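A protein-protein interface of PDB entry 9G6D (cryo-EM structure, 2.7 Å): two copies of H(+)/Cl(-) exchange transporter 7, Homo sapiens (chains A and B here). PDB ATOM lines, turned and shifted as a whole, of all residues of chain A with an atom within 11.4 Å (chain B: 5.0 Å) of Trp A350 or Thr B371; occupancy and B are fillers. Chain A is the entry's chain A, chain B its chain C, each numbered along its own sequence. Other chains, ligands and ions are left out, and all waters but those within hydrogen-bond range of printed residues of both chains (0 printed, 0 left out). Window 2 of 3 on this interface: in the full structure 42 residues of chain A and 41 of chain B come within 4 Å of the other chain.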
ATOM      1  N   PHE A 336      31.566   8.788  -9.639  1.00  0.00           N
ATOM      2  CA  PHE A 336      30.841   8.323 -10.816  1.00  0.00           C
ATOM      3  C   PHE A 336      31.761   7.588 -11.780  1.00  0.00           C
ATOM      4  O   PHE A 336      31.379   6.558 -12.346  1.00  0.00           O
ATOM      5  CB  PHE A 336      30.166   9.495 -11.524  1.00  0.00           C
ATOM      6  CG  PHE A 336      29.606   9.137 -12.868  1.00  0.00           C
ATOM      7  CD1 PHE A 336      28.461   8.366 -12.969  1.00  0.00           C
ATOM      8  CD2 PHE A 336      30.230   9.556 -14.030  1.00  0.00           C
ATOM      9  CE1 PHE A 336      27.945   8.029 -14.202  1.00  0.00           C
ATOM     10  CE2 PHE A 336      29.717   9.221 -15.266  1.00  0.00           C
ATOM     11  CZ  PHE A 336      28.573   8.456 -15.351  1.00  0.00           C
ATOM     12  N   ASN A 339      32.413   4.181 -10.427  1.00  0.00           N
ATOM     13  CA  ASN A 339      31.215   3.358 -10.552  1.00  0.00           C
ATOM     14  C   ASN A 339      30.951   2.981 -12.003  1.00  0.00           C
ATOM     15  O   ASN A 339      30.540   1.853 -12.293  1.00  0.00           O
ATOM     16  CB  ASN A 339      30.017   4.100  -9.960  1.00  0.00           C
ATOM     17  CG  ASN A 339      28.897   3.168  -9.558  1.00  0.00           C
ATOM     18  OD1 ASN A 339      28.934   1.973  -9.843  1.00  0.00           O
ATOM     19  ND2 ASN A 339      27.895   3.712  -8.879  1.00  0.00           N
ATOM     20  N   PHE A 340      31.181   3.914 -12.928  1.00  0.00           N
ATOM     21  CA  PHE A 340      30.896   3.655 -14.335  1.00  0.00           C
ATOM     22  C   PHE A 340      31.887   2.663 -14.931  1.00  0.00           C
ATOM     23  O   PHE A 340      31.494   1.718 -15.622  1.00  0.00           O
ATOM     24  CB  PHE A 340      30.910   4.967 -15.115  1.00  0.00           C
ATOM     25  CG  PHE A 340      30.788   4.794 -16.597  1.00  0.00           C
ATOM     26  CD1 PHE A 340      29.642   4.252 -17.150  1.00  0.00           C
ATOM     27  CD2 PHE A 340      31.814   5.181 -17.440  1.00  0.00           C
ATOM     28  CE1 PHE A 340      29.525   4.093 -18.515  1.00  0.00           C
ATOM     29  CE2 PHE A 340      31.702   5.025 -18.806  1.00  0.00           C
ATOM     30  CZ  PHE A 340      30.556   4.481 -19.344  1.00  0.00           C
ATOM     31  N   VAL A 341      33.182   2.864 -14.678  1.00  0.00           N
ATOM     32  CA  VAL A 341      34.199   2.027 -15.307  1.00  0.00           C
ATOM     33  C   VAL A 341      34.172   0.615 -14.733  1.00  0.00           C
ATOM     34  O   VAL A 341      34.339  -0.368 -15.466  1.00  0.00           O
ATOM     35  CB  VAL A 341      35.587   2.676 -15.166  1.00  0.00           C
ATOM     36  CG1 VAL A 341      36.674   1.718 -15.618  1.00  0.00           C
ATOM     37  CG2 VAL A 341      35.649   3.964 -15.965  1.00  0.00           C
ATOM     38  N   LEU A 342      33.962   0.484 -13.420  1.00  0.00           N
ATOM     39  CA  LEU A 342      33.856  -0.845 -12.823  1.00  0.00           C
ATOM     40  C   LEU A 342      32.685  -1.618 -13.411  1.00  0.00           C
ATOM     41  O   LEU A 342      32.765  -2.839 -13.591  1.00  0.00           O
ATOM     42  CB  LEU A 342      33.717  -0.745 -11.306  1.00  0.00           C
ATOM     43  CG  LEU A 342      34.977  -0.412 -10.511  1.00  0.00           C
ATOM     44  CD1 LEU A 342      34.699  -0.523  -9.023  1.00  0.00           C
ATOM     45  CD2 LEU A 342      36.120  -1.325 -10.914  1.00  0.00           C
ATOM     46  N   SER A 343      31.583  -0.926 -13.708  1.00  0.00           N
ATOM     47  CA  SER A 343      30.445  -1.586 -14.338  1.00  0.00           C
ATOM     48  C   SER A 343      30.813  -2.124 -15.714  1.00  0.00           C
ATOM     49  O   SER A 343      30.409  -3.233 -16.082  1.00  0.00           O
ATOM     50  CB  SER A 343      29.267  -0.617 -14.436  1.00  0.00           C
ATOM     51  OG  SER A 343      29.293   0.088 -15.663  1.00  0.00           O
ATOM     52  N   ILE A 344      31.584  -1.357 -16.486  1.00  0.00           N
ATOM     53  CA  ILE A 344      32.039  -1.837 -17.789  1.00  0.00           C
ATOM     54  C   ILE A 344      32.892  -3.087 -17.619  1.00  0.00           C
ATOM     55  O   ILE A 344      32.748  -4.063 -18.366  1.00  0.00           O
ATOM     56  CB  ILE A 344      32.807  -0.729 -18.530  1.00  0.00           C
ATOM     57  CG1 ILE A 344      31.871   0.417 -18.907  1.00  0.00           C
ATOM     58  CG2 ILE A 344      33.486  -1.287 -19.770  1.00  0.00           C
ATOM     59  CD1 ILE A 344      32.597   1.625 -19.448  1.00  0.00           C
ATOM     60  N   TYR A 345      33.790  -3.075 -16.632  1.00  0.00           N
ATOM     61  CA  TYR A 345      34.620  -4.245 -16.366  1.00  0.00           C
ATOM     62  C   TYR A 345      33.776  -5.439 -15.936  1.00  0.00           C
ATOM     63  O   TYR A 345      34.029  -6.572 -16.361  1.00  0.00           O
ATOM     64  CB  TYR A 345      35.662  -3.908 -15.300  1.00  0.00           C
ATOM     65  CG  TYR A 345      36.429  -5.103 -14.792  1.00  0.00           C
ATOM     66  CD1 TYR A 345      37.434  -5.682 -15.553  1.00  0.00           C
ATOM     67  CD2 TYR A 345      36.153  -5.650 -13.548  1.00  0.00           C
ATOM     68  CE1 TYR A 345      38.138  -6.774 -15.092  1.00  0.00           C
ATOM     69  CE2 TYR A 345      36.850  -6.740 -13.078  1.00  0.00           C
ATOM     70  CZ  TYR A 345      37.842  -7.299 -13.853  1.00  0.00           C
ATOM     71  OH  TYR A 345      38.540  -8.387 -13.387  1.00  0.00           O
ATOM     72  N   HIS A 346      32.767  -5.208 -15.100  1.00  0.00           N
ATOM     73  CA  HIS A 346      31.913  -6.279 -14.603  1.00  0.00           C
ATOM     74  C   HIS A 346      30.888  -6.753 -15.628  1.00  0.00           C
ATOM     75  O   HIS A 346      30.018  -7.558 -15.281  1.00  0.00           O
ATOM     76  CB  HIS A 346      31.196  -5.835 -13.326  1.00  0.00           C
ATOM     77  CG  HIS A 346      32.100  -5.711 -12.140  1.00  0.00           C
ATOM     78  ND1 HIS A 346      31.853  -4.835 -11.104  1.00  0.00           N
ATOM     79  CD2 HIS A 346      33.250  -6.350 -11.825  1.00  0.00           C
ATOM     80  CE1 HIS A 346      32.812  -4.942 -10.202  1.00  0.00           C
ATOM     81  NE2 HIS A 346      33.673  -5.854 -10.616  1.00  0.00           N
ATOM     82  N   GLY A 347      30.963  -6.276 -16.867  1.00  0.00           N
ATOM     83  CA  GLY A 347      30.055  -6.721 -17.903  1.00  0.00           C
ATOM     84  C   GLY A 347      28.728  -5.994 -17.906  1.00  0.00           C
ATOM     85  O   GLY A 347      28.435  -5.229 -18.829  1.00  0.00           O
ATOM     86  N   ASN A 348      27.912  -6.224 -16.879  1.00  0.00           N
ATOM     87  CA  ASN A 348      26.616  -5.565 -16.797  1.00  0.00           C
ATOM     88  C   ASN A 348      26.776  -4.064 -16.572  1.00  0.00           C
ATOM     89  O   ASN A 348      27.741  -3.607 -15.956  1.00  0.00           O
ATOM     90  CB  ASN A 348      25.742  -6.251 -15.728  1.00  0.00           C
ATOM     91  CG  ASN A 348      25.983  -5.760 -14.292  1.00  0.00           C
ATOM     92  OD1 ASN A 348      26.875  -4.968 -14.002  1.00  0.00           O
ATOM     93  ND2 ASN A 348      25.159  -6.258 -13.378  1.00  0.00           N
ATOM     94  N   MET A 349      25.847  -3.287 -17.128  1.00  0.00           N
ATOM     95  CA  MET A 349      25.996  -1.841 -17.186  1.00  0.00           C
ATOM     96  C   MET A 349      24.820  -1.070 -16.606  1.00  0.00           C
ATOM     97  O   MET A 349      24.994   0.096 -16.238  1.00  0.00           O
ATOM     98  CB  MET A 349      26.213  -1.395 -18.642  1.00  0.00           C
ATOM     99  CG  MET A 349      26.694   0.035 -18.818  1.00  0.00           C
ATOM    100  SD  MET A 349      27.951   0.168 -20.104  1.00  0.00           S
ATOM    101  CE  MET A 349      27.569   1.778 -20.787  1.00  0.00           C
ATOM    102  N   TRP A 350      23.646  -1.684 -16.490  1.00  0.00           N
ATOM    103  CA  TRP A 350      22.440  -0.992 -16.064  1.00  0.00           C
ATOM    104  C   TRP A 350      22.262  -0.980 -14.551  1.00  0.00           C
ATOM    105  O   TRP A 350      21.151  -0.733 -14.074  1.00  0.00           O
ATOM    106  CB  TRP A 350      21.213  -1.624 -16.726  1.00  0.00           C
ATOM    107  CG  TRP A 350      21.159  -1.395 -18.203  1.00  0.00           C
ATOM    108  CD1 TRP A 350      20.397  -0.476 -18.862  1.00  0.00           C
ATOM    109  CD2 TRP A 350      21.897  -2.100 -19.209  1.00  0.00           C
ATOM    110  NE1 TRP A 350      20.616  -0.562 -20.216  1.00  0.00           N
ATOM    111  CE2 TRP A 350      21.533  -1.552 -20.454  1.00  0.00           C
ATOM    112  CE3 TRP A 350      22.830  -3.140 -19.176  1.00  0.00           C
ATOM    113  CZ2 TRP A 350      22.070  -2.009 -21.656  1.00  0.00           C
ATOM    114  CZ3 TRP A 350      23.363  -3.593 -20.370  1.00  0.00           C
ATOM    115  CH2 TRP A 350      22.981  -3.028 -21.593  1.00  0.00           C
ATOM    116  N   ASP A 351      23.321  -1.248 -13.789  1.00  0.00           N
ATOM    117  CA  ASP A 351      23.260  -1.212 -12.327  1.00  0.00           C
ATOM    118  C   ASP A 351      24.591  -0.675 -11.808  1.00  0.00           C
ATOM    119  O   ASP A 351      25.578  -1.412 -11.732  1.00  0.00           O
ATOM    120  CB  ASP A 351      22.952  -2.589 -11.752  1.00  0.00           C
ATOM    121  CG  ASP A 351      23.623  -3.699 -12.527  1.00  0.00           C
ATOM    122  OD1 ASP A 351      24.476  -3.389 -13.384  1.00  0.00           O
ATOM    123  OD2 ASP A 351      23.298  -4.881 -12.283  1.00  0.00           O
ATOM    124  N   LEU A 352      24.609   0.609 -11.451  1.00  0.00           N
ATOM    125  CA  LEU A 352      25.797   1.244 -10.881  1.00  0.00           C
ATOM    126  C   LEU A 352      25.821   0.976  -9.376  1.00  0.00           C
ATOM    127  O   LEU A 352      25.529   1.836  -8.542  1.00  0.00           O
ATOM    128  CB  LEU A 352      25.807   2.733 -11.195  1.00  0.00           C
ATOM    129  CG  LEU A 352      25.834   3.155 -12.667  1.00  0.00           C
ATOM    130  CD1 LEU A 352      26.436   4.540 -12.810  1.00  0.00           C
ATOM    131  CD2 LEU A 352      26.600   2.154 -13.517  1.00  0.00           C
ATOM    132  N   SER A 353      26.181  -0.258  -9.035  1.00  0.00           N
ATOM    133  CA  SER A 353      26.073  -0.763  -7.673  1.00  0.00           C
ATOM    134  C   SER A 353      27.363  -0.628  -6.872  1.00  0.00           C
ATOM    135  O   SER A 353      27.421  -1.113  -5.738  1.00  0.00           O
ATOM    136  CB  SER A 353      25.632  -2.227  -7.694  1.00  0.00           C
ATOM    137  OG  SER A 353      26.428  -2.983  -8.589  1.00  0.00           O
ATOM    138  N   SER A 354      28.393   0.008  -7.424  1.00  0.00           N
ATOM    139  CA  SER A 354      29.677   0.170  -6.741  1.00  0.00           C
ATOM    140  C   SER A 354      30.100   1.633  -6.774  1.00  0.00           C
ATOM    141  O   SER A 354      31.016   2.013  -7.512  1.00  0.00           O
ATOM    142  CB  SER A 354      30.744  -0.722  -7.374  1.00  0.00           C
ATOM    143  OG  SER A 354      31.410  -0.050  -8.427  1.00  0.00           O
ATOM    144  N   GLU B 366      15.737  -1.627  -9.769  1.00  0.00           N
ATOM    145  CA  GLU B 366      16.355  -1.759 -11.083  1.00  0.00           C
ATOM    146  C   GLU B 366      15.698  -0.831 -12.095  1.00  0.00           C
ATOM    147  O   GLU B 366      16.348  -0.393 -13.051  1.00  0.00           O
ATOM    148  CB  GLU B 366      16.287  -3.213 -11.559  1.00  0.00           C
ATOM    149  CG  GLU B 366      14.909  -3.695 -12.017  1.00  0.00           C
ATOM    150  CD  GLU B 366      13.854  -3.650 -10.923  1.00  0.00           C
ATOM    151  OE1 GLU B 366      14.222  -3.622  -9.729  1.00  0.00           O
ATOM    152  OE2 GLU B 366      12.651  -3.639 -11.259  1.00  0.00           O
ATOM    153  N   ALA B 369      17.325   2.976 -12.310  1.00  0.00           N
ATOM    154  CA  ALA B 369      18.729   2.887 -12.677  1.00  0.00           C
ATOM    155  C   ALA B 369      18.940   3.582 -14.012  1.00  0.00           C
ATOM    156  O   ALA B 369      18.121   3.448 -14.925  1.00  0.00           O
ATOM    157  CB  ALA B 369      19.195   1.431 -12.760  1.00  0.00           C
ATOM    158  N   TYR B 370      20.039   4.320 -14.125  1.00  0.00           N
ATOM    159  CA  TYR B 370      20.324   5.106 -15.314  1.00  0.00           C
ATOM    160  C   TYR B 370      21.646   4.671 -15.933  1.00  0.00           C
ATOM    161  O   TYR B 370      22.494   4.059 -15.280  1.00  0.00           O
ATOM    162  CB  TYR B 370      20.365   6.607 -14.994  1.00  0.00           C
ATOM    163  CG  TYR B 370      21.549   7.034 -14.156  1.00  0.00           C
ATOM    164  CD1 TYR B 370      21.545   6.867 -12.779  1.00  0.00           C
ATOM    165  CD2 TYR B 370      22.665   7.616 -14.742  1.00  0.00           C
ATOM    166  CE1 TYR B 370      22.621   7.259 -12.010  1.00  0.00           C
ATOM    167  CE2 TYR B 370      23.745   8.011 -13.980  1.00  0.00           C
ATOM    168  CZ  TYR B 370      23.717   7.831 -12.615  1.00  0.00           C
ATOM    169  OH  TYR B 370      24.791   8.223 -11.850  1.00  0.00           O
ATOM    170  N   THR B 371      21.802   4.991 -17.211  1.00  0.00           N
ATOM    171  CA  THR B 371      23.013   4.718 -17.967  1.00  0.00           C
ATOM    172  C   THR B 371      23.690   6.032 -18.346  1.00  0.00           C
ATOM    173  O   THR B 371      23.182   7.123 -18.076  1.00  0.00           O
ATOM    174  CB  THR B 371      22.699   3.886 -19.211  1.00  0.00           C
ATOM    175  OG1 THR B 371      22.170   4.737 -20.234  1.00  0.00           O
ATOM    176  CG2 THR B 371      21.682   2.806 -18.885  1.00  0.00           C
ATOM    177  N   ILE B 372      24.860   5.914 -18.976  1.00  0.00           N
ATOM    178  CA  ILE B 372      25.579   7.104 -19.421  1.00  0.00           C
ATOM    179  C   ILE B 372      24.848   7.777 -20.577  1.00  0.00           C
ATOM    180  O   ILE B 372      24.958   8.994 -20.765  1.00  0.00           O
ATOM    181  CB  ILE B 372      27.030   6.742 -19.790  1.00  0.00           C
ATOM    182  CG1 ILE B 372      27.838   8.001 -20.109  1.00  0.00           C
ATOM    183  CG2 ILE B 372      27.064   5.766 -20.955  1.00  0.00           C
ATOM    184  CD1 ILE B 372      28.613   8.544 -18.933  1.00  0.00           C
ATOM    185  N   HIS B 373      24.088   7.009 -21.362  1.00  0.00           N
ATOM    186  CA  HIS B 373      23.385   7.573 -22.508  1.00  0.00           C
ATOM    187  C   HIS B 373      22.277   8.535 -22.102  1.00  0.00           C
ATOM    188  O   HIS B 373      21.872   9.370 -22.916  1.00  0.00           O
ATOM    189  CB  HIS B 373      22.808   6.451 -23.371  1.00  0.00           C
ATOM    190  CG  HIS B 373      23.846   5.556 -23.967  1.00  0.00           C
ATOM    191  ND1 HIS B 373      24.118   4.298 -23.472  1.00  0.00           N
ATOM    192  CD2 HIS B 373      24.683   5.735 -25.017  1.00  0.00           C
ATOM    193  CE1 HIS B 373      25.077   3.742 -24.192  1.00  0.00           C
ATOM    194  NE2 HIS B 373      25.436   4.592 -25.136  1.00  0.00           N
ATOM    195  N   GLU B 374      21.778   8.439 -20.870  1.00  0.00           N
ATOM    196  CA  GLU B 374      20.733   9.338 -20.402  1.00  0.00           C
ATOM    197  C   GLU B 374      21.278  10.644 -19.841  1.00  0.00           C
ATOM    198  O   GLU B 374      20.482  11.525 -19.499  1.00  0.00           O
ATOM    199  CB  GLU B 374      19.880   8.648 -19.339  1.00  0.00           C
ATOM    200  CG  GLU B 374      19.182   7.397 -19.827  1.00  0.00           C
ATOM    201  CD  GLU B 374      18.733   6.505 -18.690  1.00  0.00           C
ATOM    202  OE1 GLU B 374      17.829   6.916 -17.933  1.00  0.00           O
ATOM    203  OE2 GLU B 374      19.284   5.393 -18.552  1.00  0.00           O
ATOM    204  N   ILE B 375      22.599  10.787 -19.730  1.00  0.00           N
ATOM    205  CA  ILE B 375      23.168  12.034 -19.214  1.00  0.00           C
ATOM    206  C   ILE B 375      22.792  13.234 -20.076  1.00  0.00           C
ATOM    207  O   ILE B 375      22.368  14.258 -19.514  1.00  0.00           O
ATOM    208  CB  ILE B 375      24.689  11.885 -19.030  1.00  0.00           C
ATOM    209  CG1 ILE B 375      25.002  10.900 -17.901  1.00  0.00           C
ATOM    210  CG2 ILE B 375      25.328  13.235 -18.751  1.00  0.00           C
ATOM    211  CD1 ILE B 375      24.149  11.086 -16.668  1.00  0.00           C
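Trp A350 touches just these residues of chain B: Ala B369 and Thr B371. Thr B371 touches just one residue of chain A: Trp A350. No residue of chain A comes within 4 Å of Glu B374. No residue of chain A comes within 4 Å of Ile B375. Of the printed residues of chain B, Phe A340 touches Ile B372 (3.8 Å). Of the printed residues of chain B, Phe A336 touches Tyr B370 (3.8 Å) and Ile B372 (3.6 Å). Glu B366 touches none of the printed residues of chain A. Leu A352 touches none of the printed residues of chain B.
No position is printed for both chains. Of the 5 pairs that touch across the chains among the printed residues, none has its exchanged pair printed and touching as well.
Among the printed residues, pairs that only touch across the chains: Phe A336 with Tyr B370, Phe A336 with Ile B372, Phe A340 with Ile B372, Trp A350 with Ala B369 and Trp A350 with Thr B371.
Hydrophobic or aromatic side chains of chain A within 4 Å of the printed part of chain B: Phe A336, Phe A340 and Trp A350. Printed residues of chain B that touch a printed residue of chain A: Ala B369, Tyr B370, Thr B371 and Ile B372.
The side-chain hydroxyl (OG) of Ser A343 lies within hydrogen-bond range of the backbone carbonyl oxygen (O) of Phe A340, at 2.7 Å. OE2 of Glu B374 sits at hydrogen-bond distance from N of Thr B371 (2.9 Å). N of His B373 lies within hydrogen-bond range of OG1 of Thr B371, at 3.2 Å.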
